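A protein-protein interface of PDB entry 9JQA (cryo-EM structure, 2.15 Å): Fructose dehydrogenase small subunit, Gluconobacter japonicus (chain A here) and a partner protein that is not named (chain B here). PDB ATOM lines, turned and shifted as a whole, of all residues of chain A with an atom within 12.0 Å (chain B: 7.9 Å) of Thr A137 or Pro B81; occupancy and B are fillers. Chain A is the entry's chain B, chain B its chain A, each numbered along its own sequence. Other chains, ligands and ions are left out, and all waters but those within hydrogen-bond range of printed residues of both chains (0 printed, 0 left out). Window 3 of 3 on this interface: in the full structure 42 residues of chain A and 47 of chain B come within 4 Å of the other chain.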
ATOM      1  N   GLN A  82      17.538  17.269  -2.940  1.00  0.00           N
ATOM      2  CA  GLN A  82      18.859  16.649  -2.888  1.00  0.00           C
ATOM      3  C   GLN A  82      19.741  17.117  -4.036  1.00  0.00           C
ATOM      4  O   GLN A  82      20.909  17.469  -3.830  1.00  0.00           O
ATOM      5  CB  GLN A  82      18.711  15.130  -2.919  1.00  0.00           C
ATOM      6  CG  GLN A  82      19.809  14.365  -2.215  1.00  0.00           C
ATOM      7  CD  GLN A  82      19.619  12.868  -2.331  1.00  0.00           C
ATOM      8  OE1 GLN A  82      19.246  12.361  -3.386  1.00  0.00           O
ATOM      9  NE2 GLN A  82      19.869  12.153  -1.242  1.00  0.00           N
ATOM     10  N   SER A 130      12.375   0.847  -2.491  1.00  0.00           N
ATOM     11  CA  SER A 130      12.612   0.824  -1.055  1.00  0.00           C
ATOM     12  C   SER A 130      11.847   1.899  -0.300  1.00  0.00           C
ATOM     13  O   SER A 130      11.676   1.776   0.917  1.00  0.00           O
ATOM     14  CB  SER A 130      14.106   0.981  -0.769  1.00  0.00           C
ATOM     15  OG  SER A 130      14.585   2.217  -1.260  1.00  0.00           O
ATOM     16  N   GLY A 131      11.385   2.941  -0.982  1.00  0.00           N
ATOM     17  CA  GLY A 131      10.688   4.022  -0.326  1.00  0.00           C
ATOM     18  C   GLY A 131      11.573   5.073   0.302  1.00  0.00           C
ATOM     19  O   GLY A 131      11.050   5.990   0.944  1.00  0.00           O
ATOM     20  N   VAL A 132      12.893   4.973   0.145  1.00  0.00           N
ATOM     21  CA  VAL A 132      13.823   5.947   0.694  1.00  0.00           C
ATOM     22  C   VAL A 132      14.763   6.406  -0.408  1.00  0.00           C
ATOM     23  O   VAL A 132      14.974   5.719  -1.409  1.00  0.00           O
ATOM     24  CB  VAL A 132      14.638   5.392   1.881  1.00  0.00           C
ATOM     25  CG1 VAL A 132      13.767   5.260   3.107  1.00  0.00           C
ATOM     26  CG2 VAL A 132      15.268   4.066   1.518  1.00  0.00           C
ATOM     27  N   ILE A 133      15.337   7.587  -0.202  1.00  0.00           N
ATOM     28  CA  ILE A 133      16.294   8.168  -1.126  1.00  0.00           C
ATOM     29  C   ILE A 133      17.705   8.160  -0.550  1.00  0.00           C
ATOM     30  O   ILE A 133      18.669   7.891  -1.269  1.00  0.00           O
ATOM     31  CB  ILE A 133      15.860   9.596  -1.519  1.00  0.00           C
ATOM     32  CG1 ILE A 133      14.598   9.532  -2.376  1.00  0.00           C
ATOM     33  CG2 ILE A 133      16.966  10.315  -2.256  1.00  0.00           C
ATOM     34  CD1 ILE A 133      14.142  10.864  -2.881  1.00  0.00           C
ATOM     35  N   GLU A 134      17.843   8.432   0.741  1.00  0.00           N
ATOM     36  CA  GLU A 134      19.132   8.379   1.407  1.00  0.00           C
ATOM     37  C   GLU A 134      19.337   7.015   2.059  1.00  0.00           C
ATOM     38  O   GLU A 134      18.415   6.206   2.177  1.00  0.00           O
ATOM     39  CB  GLU A 134      19.241   9.492   2.446  1.00  0.00           C
ATOM     40  CG  GLU A 134      19.835  10.777   1.906  1.00  0.00           C
ATOM     41  CD  GLU A 134      18.990  11.986   2.231  1.00  0.00           C
ATOM     42  OE1 GLU A 134      18.428  12.036   3.345  1.00  0.00           O
ATOM     43  OE2 GLU A 134      18.885  12.888   1.374  1.00  0.00           O
ATOM     44  N   ASP A 135      20.569   6.766   2.492  1.00  0.00           N
ATOM     45  CA  ASP A 135      20.966   5.484   3.064  1.00  0.00           C
ATOM     46  C   ASP A 135      21.334   5.611   4.538  1.00  0.00           C
ATOM     47  O   ASP A 135      22.273   4.972   5.016  1.00  0.00           O
ATOM     48  CB  ASP A 135      22.129   4.884   2.280  1.00  0.00           C
ATOM     49  CG  ASP A 135      23.152   5.925   1.874  1.00  0.00           C
ATOM     50  OD1 ASP A 135      22.745   7.039   1.482  1.00  0.00           O
ATOM     51  OD2 ASP A 135      24.364   5.630   1.947  1.00  0.00           O
ATOM     52  N   GLU A 136      20.597   6.429   5.278  1.00  0.00           N
ATOM     53  CA  GLU A 136      20.834   6.643   6.696  1.00  0.00           C
ATOM     54  C   GLU A 136      19.693   6.042   7.512  1.00  0.00           C
ATOM     55  O   GLU A 136      18.751   5.452   6.977  1.00  0.00           O
ATOM     56  CB  GLU A 136      20.992   8.134   6.996  1.00  0.00           C
ATOM     57  CG  GLU A 136      21.878   8.875   6.014  1.00  0.00           C
ATOM     58  CD  GLU A 136      21.320  10.233   5.640  1.00  0.00           C
ATOM     59  OE1 GLU A 136      20.080  10.379   5.611  1.00  0.00           O
ATOM     60  OE2 GLU A 136      22.120  11.155   5.380  1.00  0.00           O
ATOM     61  N   THR A 137      19.796   6.195   8.832  1.00  0.00           N
ATOM     62  CA  THR A 137      18.743   5.779   9.748  1.00  0.00           C
ATOM     63  C   THR A 137      17.657   6.837   9.891  1.00  0.00           C
ATOM     64  O   THR A 137      16.493   6.499  10.133  1.00  0.00           O
ATOM     65  CB  THR A 137      19.349   5.456  11.120  1.00  0.00           C
ATOM     66  OG1 THR A 137      20.255   4.354  10.993  1.00  0.00           O
ATOM     67  CG2 THR A 137      18.272   5.100  12.135  1.00  0.00           C
ATOM     68  N   ASN A 138      18.007   8.107   9.721  1.00  0.00           N
ATOM     69  CA  ASN A 138      17.052   9.200   9.786  1.00  0.00           C
ATOM     70  C   ASN A 138      16.438   9.522   8.430  1.00  0.00           C
ATOM     71  O   ASN A 138      15.705  10.508   8.315  1.00  0.00           O
ATOM     72  CB  ASN A 138      17.722  10.449  10.358  1.00  0.00           C
ATOM     73  CG  ASN A 138      18.953  10.855   9.573  1.00  0.00           C
ATOM     74  OD1 ASN A 138      19.914  10.093   9.467  1.00  0.00           O
ATOM     75  ND2 ASN A 138      18.927  12.057   9.013  1.00  0.00           N
ATOM     76  N   ALA A 139      16.735   8.725   7.406  1.00  0.00           N
ATOM     77  CA  ALA A 139      16.207   8.985   6.075  1.00  0.00           C
ATOM     78  C   ALA A 139      14.686   8.933   6.081  1.00  0.00           C
ATOM     79  O   ALA A 139      14.079   8.088   6.744  1.00  0.00           O
ATOM     80  CB  ALA A 139      16.764   7.972   5.076  1.00  0.00           C
ATOM     81  N   LYS A 140      14.073   9.850   5.342  1.00  0.00           N
ATOM     82  CA  LYS A 140      12.621   9.900   5.265  1.00  0.00           C
ATOM     83  C   LYS A 140      12.102   8.743   4.424  1.00  0.00           C
ATOM     84  O   LYS A 140      12.609   8.477   3.331  1.00  0.00           O
ATOM     85  CB  LYS A 140      12.170  11.232   4.670  1.00  0.00           C
ATOM     86  CG  LYS A 140      12.717  12.449   5.392  1.00  0.00           C
ATOM     87  CD  LYS A 140      11.914  13.708   5.091  1.00  0.00           C
ATOM     88  CE  LYS A 140      10.461  13.397   4.764  1.00  0.00           C
ATOM     89  NZ  LYS A 140       9.813  14.484   3.980  1.00  0.00           N
ATOM     90  N   VAL A 141      11.091   8.052   4.937  1.00  0.00           N
ATOM     91  CA  VAL A 141      10.429   6.985   4.200  1.00  0.00           C
ATOM     92  C   VAL A 141       9.240   7.587   3.469  1.00  0.00           C
ATOM     93  O   VAL A 141       8.316   8.115   4.095  1.00  0.00           O
ATOM     94  CB  VAL A 141       9.988   5.850   5.134  1.00  0.00           C
ATOM     95  CG1 VAL A 141       8.989   4.949   4.437  1.00  0.00           C
ATOM     96  CG2 VAL A 141      11.186   5.051   5.586  1.00  0.00           C
ATOM     97  N   TYR A 142       9.270   7.527   2.145  1.00  0.00           N
ATOM     98  CA  TYR A 142       8.182   8.053   1.338  1.00  0.00           C
ATOM     99  C   TYR A 142       7.172   6.988   0.949  1.00  0.00           C
ATOM    100  O   TYR A 142       6.110   7.330   0.424  1.00  0.00           O
ATOM    101  CB  TYR A 142       8.746   8.727   0.086  1.00  0.00           C
ATOM    102  CG  TYR A 142       9.727   9.816   0.424  1.00  0.00           C
ATOM    103  CD1 TYR A 142       9.292  11.101   0.701  1.00  0.00           C
ATOM    104  CD2 TYR A 142      11.085   9.552   0.508  1.00  0.00           C
ATOM    105  CE1 TYR A 142      10.180  12.096   1.030  1.00  0.00           C
ATOM    106  CE2 TYR A 142      11.981  10.542   0.837  1.00  0.00           C
ATOM    107  CZ  TYR A 142      11.523  11.812   1.097  1.00  0.00           C
ATOM    108  OH  TYR A 142      12.416  12.800   1.428  1.00  0.00           O
ATOM    109  N   ASN B  53       7.655   3.981   9.282  1.00  0.00           N
ATOM    110  CA  ASN B  53       8.458   5.025   8.668  1.00  0.00           C
ATOM    111  C   ASN B  53       9.941   4.883   8.977  1.00  0.00           C
ATOM    112  O   ASN B  53      10.721   5.772   8.630  1.00  0.00           O
ATOM    113  CB  ASN B  53       7.956   6.399   9.108  1.00  0.00           C
ATOM    114  CG  ASN B  53       6.892   6.944   8.185  1.00  0.00           C
ATOM    115  OD1 ASN B  53       5.735   6.536   8.246  1.00  0.00           O
ATOM    116  ND2 ASN B  53       7.278   7.868   7.317  1.00  0.00           N
ATOM    117  N   MET B  54      10.339   3.804   9.638  1.00  0.00           N
ATOM    118  CA  MET B  54      11.751   3.492   9.770  1.00  0.00           C
ATOM    119  C   MET B  54      12.301   3.031   8.422  1.00  0.00           C
ATOM    120  O   MET B  54      11.602   2.347   7.670  1.00  0.00           O
ATOM    121  CB  MET B  54      11.950   2.414  10.834  1.00  0.00           C
ATOM    122  CG  MET B  54      13.303   2.422  11.517  1.00  0.00           C
ATOM    123  SD  MET B  54      13.509   1.014  12.615  1.00  0.00           S
ATOM    124  CE  MET B  54      13.108  -0.322  11.506  1.00  0.00           C
ATOM    125  N   PRO B  55      13.533   3.405   8.079  1.00  0.00           N
ATOM    126  CA  PRO B  55      14.060   3.053   6.765  1.00  0.00           C
ATOM    127  C   PRO B  55      14.122   1.550   6.588  1.00  0.00           C
ATOM    128  O   PRO B  55      14.323   0.797   7.559  1.00  0.00           O
ATOM    129  CB  PRO B  55      15.461   3.679   6.771  1.00  0.00           C
ATOM    130  CG  PRO B  55      15.341   4.809   7.703  1.00  0.00           C
ATOM    131  CD  PRO B  55      14.412   4.352   8.782  1.00  0.00           C
ATOM    132  N   PRO B  56      13.945   1.064   5.357  1.00  0.00           N
ATOM    133  CA  PRO B  56      13.927  -0.389   5.135  1.00  0.00           C
ATOM    134  C   PRO B  56      15.224  -1.084   5.497  1.00  0.00           C
ATOM    135  O   PRO B  56      15.203  -2.284   5.786  1.00  0.00           O
ATOM    136  CB  PRO B  56      13.626  -0.503   3.636  1.00  0.00           C
ATOM    137  CG  PRO B  56      14.074   0.786   3.064  1.00  0.00           C
ATOM    138  CD  PRO B  56      13.775   1.812   4.104  1.00  0.00           C
ATOM    139  N   ASP B  57      16.357  -0.383   5.466  1.00  0.00           N
ATOM    140  CA  ASP B  57      17.597  -0.994   5.929  1.00  0.00           C
ATOM    141  C   ASP B  57      17.543  -1.290   7.419  1.00  0.00           C
ATOM    142  O   ASP B  57      18.138  -2.269   7.878  1.00  0.00           O
ATOM    143  CB  ASP B  57      18.784  -0.090   5.610  1.00  0.00           C
ATOM    144  CG  ASP B  57      19.607  -0.603   4.453  1.00  0.00           C
ATOM    145  OD1 ASP B  57      19.794  -1.833   4.356  1.00  0.00           O
ATOM    146  OD2 ASP B  57      20.069   0.222   3.639  1.00  0.00           O
ATOM    147  N   ASN B  58      16.840  -0.457   8.184  1.00  0.00           N
ATOM    148  CA  ASN B  58      16.649  -0.713   9.601  1.00  0.00           C
ATOM    149  C   ASN B  58      15.609  -1.791   9.866  1.00  0.00           C
ATOM    150  O   ASN B  58      15.524  -2.283  10.992  1.00  0.00           O
ATOM    151  CB  ASN B  58      16.248   0.577  10.313  1.00  0.00           C
ATOM    152  CG  ASN B  58      17.351   1.608  10.309  1.00  0.00           C
ATOM    153  OD1 ASN B  58      17.745   2.109   9.260  1.00  0.00           O
ATOM    154  ND2 ASN B  58      17.852   1.936  11.489  1.00  0.00           N
ATOM    155  N   ASP B  63      16.533  -3.653  13.681  1.00  0.00           N
ATOM    156  CA  ASP B  63      16.496  -2.454  14.512  1.00  0.00           C
ATOM    157  C   ASP B  63      15.229  -2.487  15.352  1.00  0.00           C
ATOM    158  O   ASP B  63      14.128  -2.260  14.841  1.00  0.00           O
ATOM    159  CB  ASP B  63      16.551  -1.195  13.654  1.00  0.00           C
ATOM    160  CG  ASP B  63      16.792   0.059  14.466  1.00  0.00           C
ATOM    161  OD1 ASP B  63      16.759  -0.005  15.710  1.00  0.00           O
ATOM    162  OD2 ASP B  63      17.021   1.120  13.856  1.00  0.00           O
ATOM    163  N   THR B  66      14.839   1.960  17.302  1.00  0.00           N
ATOM    164  CA  THR B  66      14.491   3.214  16.638  1.00  0.00           C
ATOM    165  C   THR B  66      13.011   3.572  16.737  1.00  0.00           C
ATOM    166  O   THR B  66      12.711   4.759  16.951  1.00  0.00           O
ATOM    167  CB  THR B  66      14.945   3.163  15.174  1.00  0.00           C
ATOM    168  OG1 THR B  66      16.370   3.049  15.126  1.00  0.00           O
ATOM    169  CG2 THR B  66      14.527   4.417  14.433  1.00  0.00           C
ATOM    170  N   HIS B  76      17.871   4.735  26.440  1.00  0.00           N
ATOM    171  CA  HIS B  76      18.000   3.299  26.276  1.00  0.00           C
ATOM    172  C   HIS B  76      18.890   3.016  25.075  1.00  0.00           C
ATOM    173  O   HIS B  76      19.313   3.923  24.358  1.00  0.00           O
ATOM    174  CB  HIS B  76      16.632   2.618  26.132  1.00  0.00           C
ATOM    175  CG  HIS B  76      15.791   3.151  25.015  1.00  0.00           C
ATOM    176  ND1 HIS B  76      16.094   2.942  23.688  1.00  0.00           N
ATOM    177  CD2 HIS B  76      14.640   3.863  25.030  1.00  0.00           C
ATOM    178  CE1 HIS B  76      15.175   3.513  22.933  1.00  0.00           C
ATOM    179  NE2 HIS B  76      14.281   4.079  23.723  1.00  0.00           N
ATOM    180  N   THR B  77      19.184   1.739  24.867  1.00  0.00           N
ATOM    181  CA  THR B  77      20.187   1.349  23.887  1.00  0.00           C
ATOM    182  C   THR B  77      19.635   1.441  22.471  1.00  0.00           C
ATOM    183  O   THR B  77      18.531   0.969  22.190  1.00  0.00           O
ATOM    184  CB  THR B  77      20.675  -0.069  24.164  1.00  0.00           C
ATOM    185  OG1 THR B  77      19.552  -0.951  24.249  1.00  0.00           O
ATOM    186  CG2 THR B  77      21.439  -0.112  25.467  1.00  0.00           C
ATOM    187  N   ASN B  78      20.411   2.057  21.587  1.00  0.00           N
ATOM    188  CA  ASN B  78      20.164   2.060  20.155  1.00  0.00           C
ATOM    189  C   ASN B  78      21.472   1.716  19.465  1.00  0.00           C
ATOM    190  O   ASN B  78      22.535   2.188  19.874  1.00  0.00           O
ATOM    191  CB  ASN B  78      19.639   3.416  19.675  1.00  0.00           C
ATOM    192  CG  ASN B  78      19.045   3.352  18.286  1.00  0.00           C
ATOM    193  OD1 ASN B  78      19.764   3.257  17.295  1.00  0.00           O
ATOM    194  ND2 ASN B  78      17.724   3.409  18.206  1.00  0.00           N
ATOM    195  N   TYR B  79      21.403   0.887  18.428  1.00  0.00           N
ATOM    196  CA  TYR B  79      22.608   0.297  17.873  1.00  0.00           C
ATOM    197  C   TYR B  79      22.814   0.533  16.387  1.00  0.00           C
ATOM    198  O   TYR B  79      23.875   0.164  15.871  1.00  0.00           O
ATOM    199  CB  TYR B  79      22.631  -1.215  18.143  1.00  0.00           C
ATOM    200  CG  TYR B  79      22.784  -1.527  19.606  1.00  0.00           C
ATOM    201  CD1 TYR B  79      23.975  -1.267  20.264  1.00  0.00           C
ATOM    202  CD2 TYR B  79      21.731  -2.049  20.335  1.00  0.00           C
ATOM    203  CE1 TYR B  79      24.117  -1.534  21.600  1.00  0.00           C
ATOM    204  CE2 TYR B  79      21.867  -2.321  21.672  1.00  0.00           C
ATOM    205  CZ  TYR B  79      23.061  -2.061  22.301  1.00  0.00           C
ATOM    206  OH  TYR B  79      23.202  -2.327  23.638  1.00  0.00           O
ATOM    207  N   PHE B  80      21.860   1.113  15.684  1.00  0.00           N
ATOM    208  CA  PHE B  80      22.135   1.295  14.268  1.00  0.00           C
ATOM    209  C   PHE B  80      23.016   2.525  14.086  1.00  0.00           C
ATOM    210  O   PHE B  80      24.072   2.426  13.447  1.00  0.00           O
ATOM    211  CB  PHE B  80      20.835   1.321  13.469  1.00  0.00           C
ATOM    212  CG  PHE B  80      20.362  -0.046  13.117  1.00  0.00           C
ATOM    213  CD1 PHE B  80      20.265  -1.014  14.100  1.00  0.00           C
ATOM    214  CD2 PHE B  80      20.078  -0.389  11.814  1.00  0.00           C
ATOM    215  CE1 PHE B  80      19.868  -2.282  13.799  1.00  0.00           C
ATOM    216  CE2 PHE B  80      19.668  -1.662  11.507  1.00  0.00           C
ATOM    217  CZ  PHE B  80      19.561  -2.608  12.506  1.00  0.00           C
ATOM    218  N   PRO B  81      22.647   3.693  14.609  1.00  0.00           N
ATOM    219  CA  PRO B  81      23.687   4.568  15.153  1.00  0.00           C
ATOM    220  C   PRO B  81      23.910   4.190  16.606  1.00  0.00           C
ATOM    221  O   PRO B  81      23.025   4.417  17.436  1.00  0.00           O
ATOM    222  CB  PRO B  81      23.104   5.978  14.995  1.00  0.00           C
ATOM    223  CG  PRO B  81      21.748   5.797  14.352  1.00  0.00           C
ATOM    224  CD  PRO B  81      21.349   4.382  14.570  1.00  0.00           C
ATOM    225  N   ASP B  82      25.063   3.611  16.936  1.00  0.00           N
ATOM    226  CA  ASP B  82      25.318   3.214  18.316  1.00  0.00           C
ATOM    227  C   ASP B  82      25.330   4.449  19.205  1.00  0.00           C
ATOM    228  O   ASP B  82      26.229   5.288  19.099  1.00  0.00           O
ATOM    229  CB  ASP B  82      26.639   2.451  18.428  1.00  0.00           C
ATOM    230  CG  ASP B  82      26.768   1.690  19.736  1.00  0.00           C
ATOM    231  OD1 ASP B  82      25.994   1.962  20.675  1.00  0.00           O
ATOM    232  OD2 ASP B  82      27.651   0.815  19.828  1.00  0.00           O
ATOM    233  N   ASN B  83      24.335   4.570  20.079  1.00  0.00           N
ATOM    234  CA  ASN B  83      24.187   5.767  20.894  1.00  0.00           C
ATOM    235  C   ASN B  83      25.110   5.773  22.103  1.00  0.00           C
ATOM    236  O   ASN B  83      25.110   6.756  22.851  1.00  0.00           O
ATOM    237  CB  ASN B  83      22.731   5.932  21.337  1.00  0.00           C
ATOM    238  CG  ASN B  83      22.262   4.818  22.244  1.00  0.00           C
ATOM    239  OD1 ASN B  83      22.828   3.729  22.255  1.00  0.00           O
ATOM    240  ND2 ASN B  83      21.213   5.086  23.006  1.00  0.00           N
ATOM    241  N   ASN B  84      25.884   4.707  22.306  1.00  0.00           N
ATOM    242  CA  ASN B  84      26.919   4.656  23.336  1.00  0.00           C
ATOM    243  C   ASN B  84      26.341   4.846  24.736  1.00  0.00           C
ATOM    244  O   ASN B  84      26.976   5.443  25.606  1.00  0.00           O
ATOM    245  CB  ASN B  84      28.019   5.685  23.057  1.00  0.00           C
ATOM    246  CG  ASN B  84      29.279   5.426  23.853  1.00  0.00           C
ATOM    247  OD1 ASN B  84      29.627   6.188  24.754  1.00  0.00           O
ATOM    248  ND2 ASN B  84      29.969   4.339  23.530  1.00  0.00           N
ATOM    249  N   TYR B  85      25.131   4.345  24.972  1.00  0.00           N
ATOM    250  CA  TYR B  85      24.587   4.375  26.324  1.00  0.00           C
ATOM    251  C   TYR B  85      25.152   3.233  27.156  1.00  0.00           C
ATOM    252  O   TYR B  85      25.771   3.455  28.200  1.00  0.00           O
ATOM    253  CB  TYR B  85      23.060   4.309  26.296  1.00  0.00           C
ATOM    254  CG  TYR B  85      22.475   4.113  27.673  1.00  0.00           C
ATOM    255  CD1 TYR B  85      22.614   5.089  28.646  1.00  0.00           C
ATOM    256  CD2 TYR B  85      21.814   2.944  28.007  1.00  0.00           C
ATOM    257  CE1 TYR B  85      22.097   4.914  29.906  1.00  0.00           C
ATOM    258  CE2 TYR B  85      21.295   2.759  29.266  1.00  0.00           C
ATOM    259  CZ  TYR B  85      21.439   3.749  30.212  1.00  0.00           C
ATOM    260  OH  TYR B  85      20.921   3.573  31.470  1.00  0.00           O
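ND2 of Asn B53 is in hydrogen-bond range of O of Val A141 (3.4 Å). ND2 of Asn B58 lies close to OG1 of Thr A137 (3.4 Å).
The side-chain amide oxygen (OD1) of Asn B78 sits close to the backbone carbonyl oxygen (O) of Pro B81 (3.5 Å). The side-chain amide oxygen (OD1) of Asn B78 lies within hydrogen-bond range of the backbone NH (N) of Phe B80 (3.4 Å). The side-chain carboxylate (OD2) of Asp B63 lies within hydrogen-bond range of the side-chain amide nitrogen (ND2) of Asn B58.
O of Ser A130 touches CG of Pro B56, at 3.4 Å. CG1 of Val A132 touches CD of Pro B56, at 3.6 Å. Glu A136 touches Pro B55. CG of Pro B55 touches O of Thr A137, 3.2 Å away. Phe B80 touches Thr A137. Thr A137 touches Pro B81 (OG1 to CD, 3.7 Å). CG of Pro B55 touches O of Ala A139, at 3.6 Å. Val A141 touches Met B54 (CG2 to O, 3.4 Å). Pro B55 touches Val A141.
Of the printed residues of chain A, Pro B81 touches Thr A137. Met B54 touches one residue of chain A. Of chain A, only Glu A136, Thr A137, Ala A139 and Val A141 come within 4 Å of Pro B55. No residue of chain A comes within 4 Å of Asn B78. No residue of chain A comes within 4 Å of Asp B82. No residue of chain A comes within 4 Å of Asn B83. Printed residues of chain B within 4 Å of Ala A139: Pro B55 (3.6 Å). Of the printed residues of chain B, Glu A136 touches Pro B55 (3.5 Å). Printed residues of chain B within 4 Å of Ser A130: Pro B56. Printed residues of chain B within 4 Å of Val A141: Asn B53, Met B54 and Pro B55. Asn B84 touches none of the printed residues of chain A. The nearest residue of chain B that does not touch Thr A137 is Thr B66 (4.1 Å). The nearest printed residue of chain A that does not touch Asn B58 is Glu A136 (4.2 Å).
Printed residues of chain B that touch a printed residue of chain A: Asn B53, Met B54, Pro B55, Pro B56, Asn B58, Phe B80 and Pro B81. Hydrophobic or aromatic side chains of chain B that line the printed part of chain A: Pro B55, Pro B56, Phe B80 and Pro B81. Of the 14 printed residues of chain A, 6 touch a printed residue of chain B. Among the printed residues, 11 pairs touch across the chains. Among the printed residues, no Asp or Glu carboxylate lies within 4 Å of a Lys or Arg side-chain nitrogen of the other chain.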
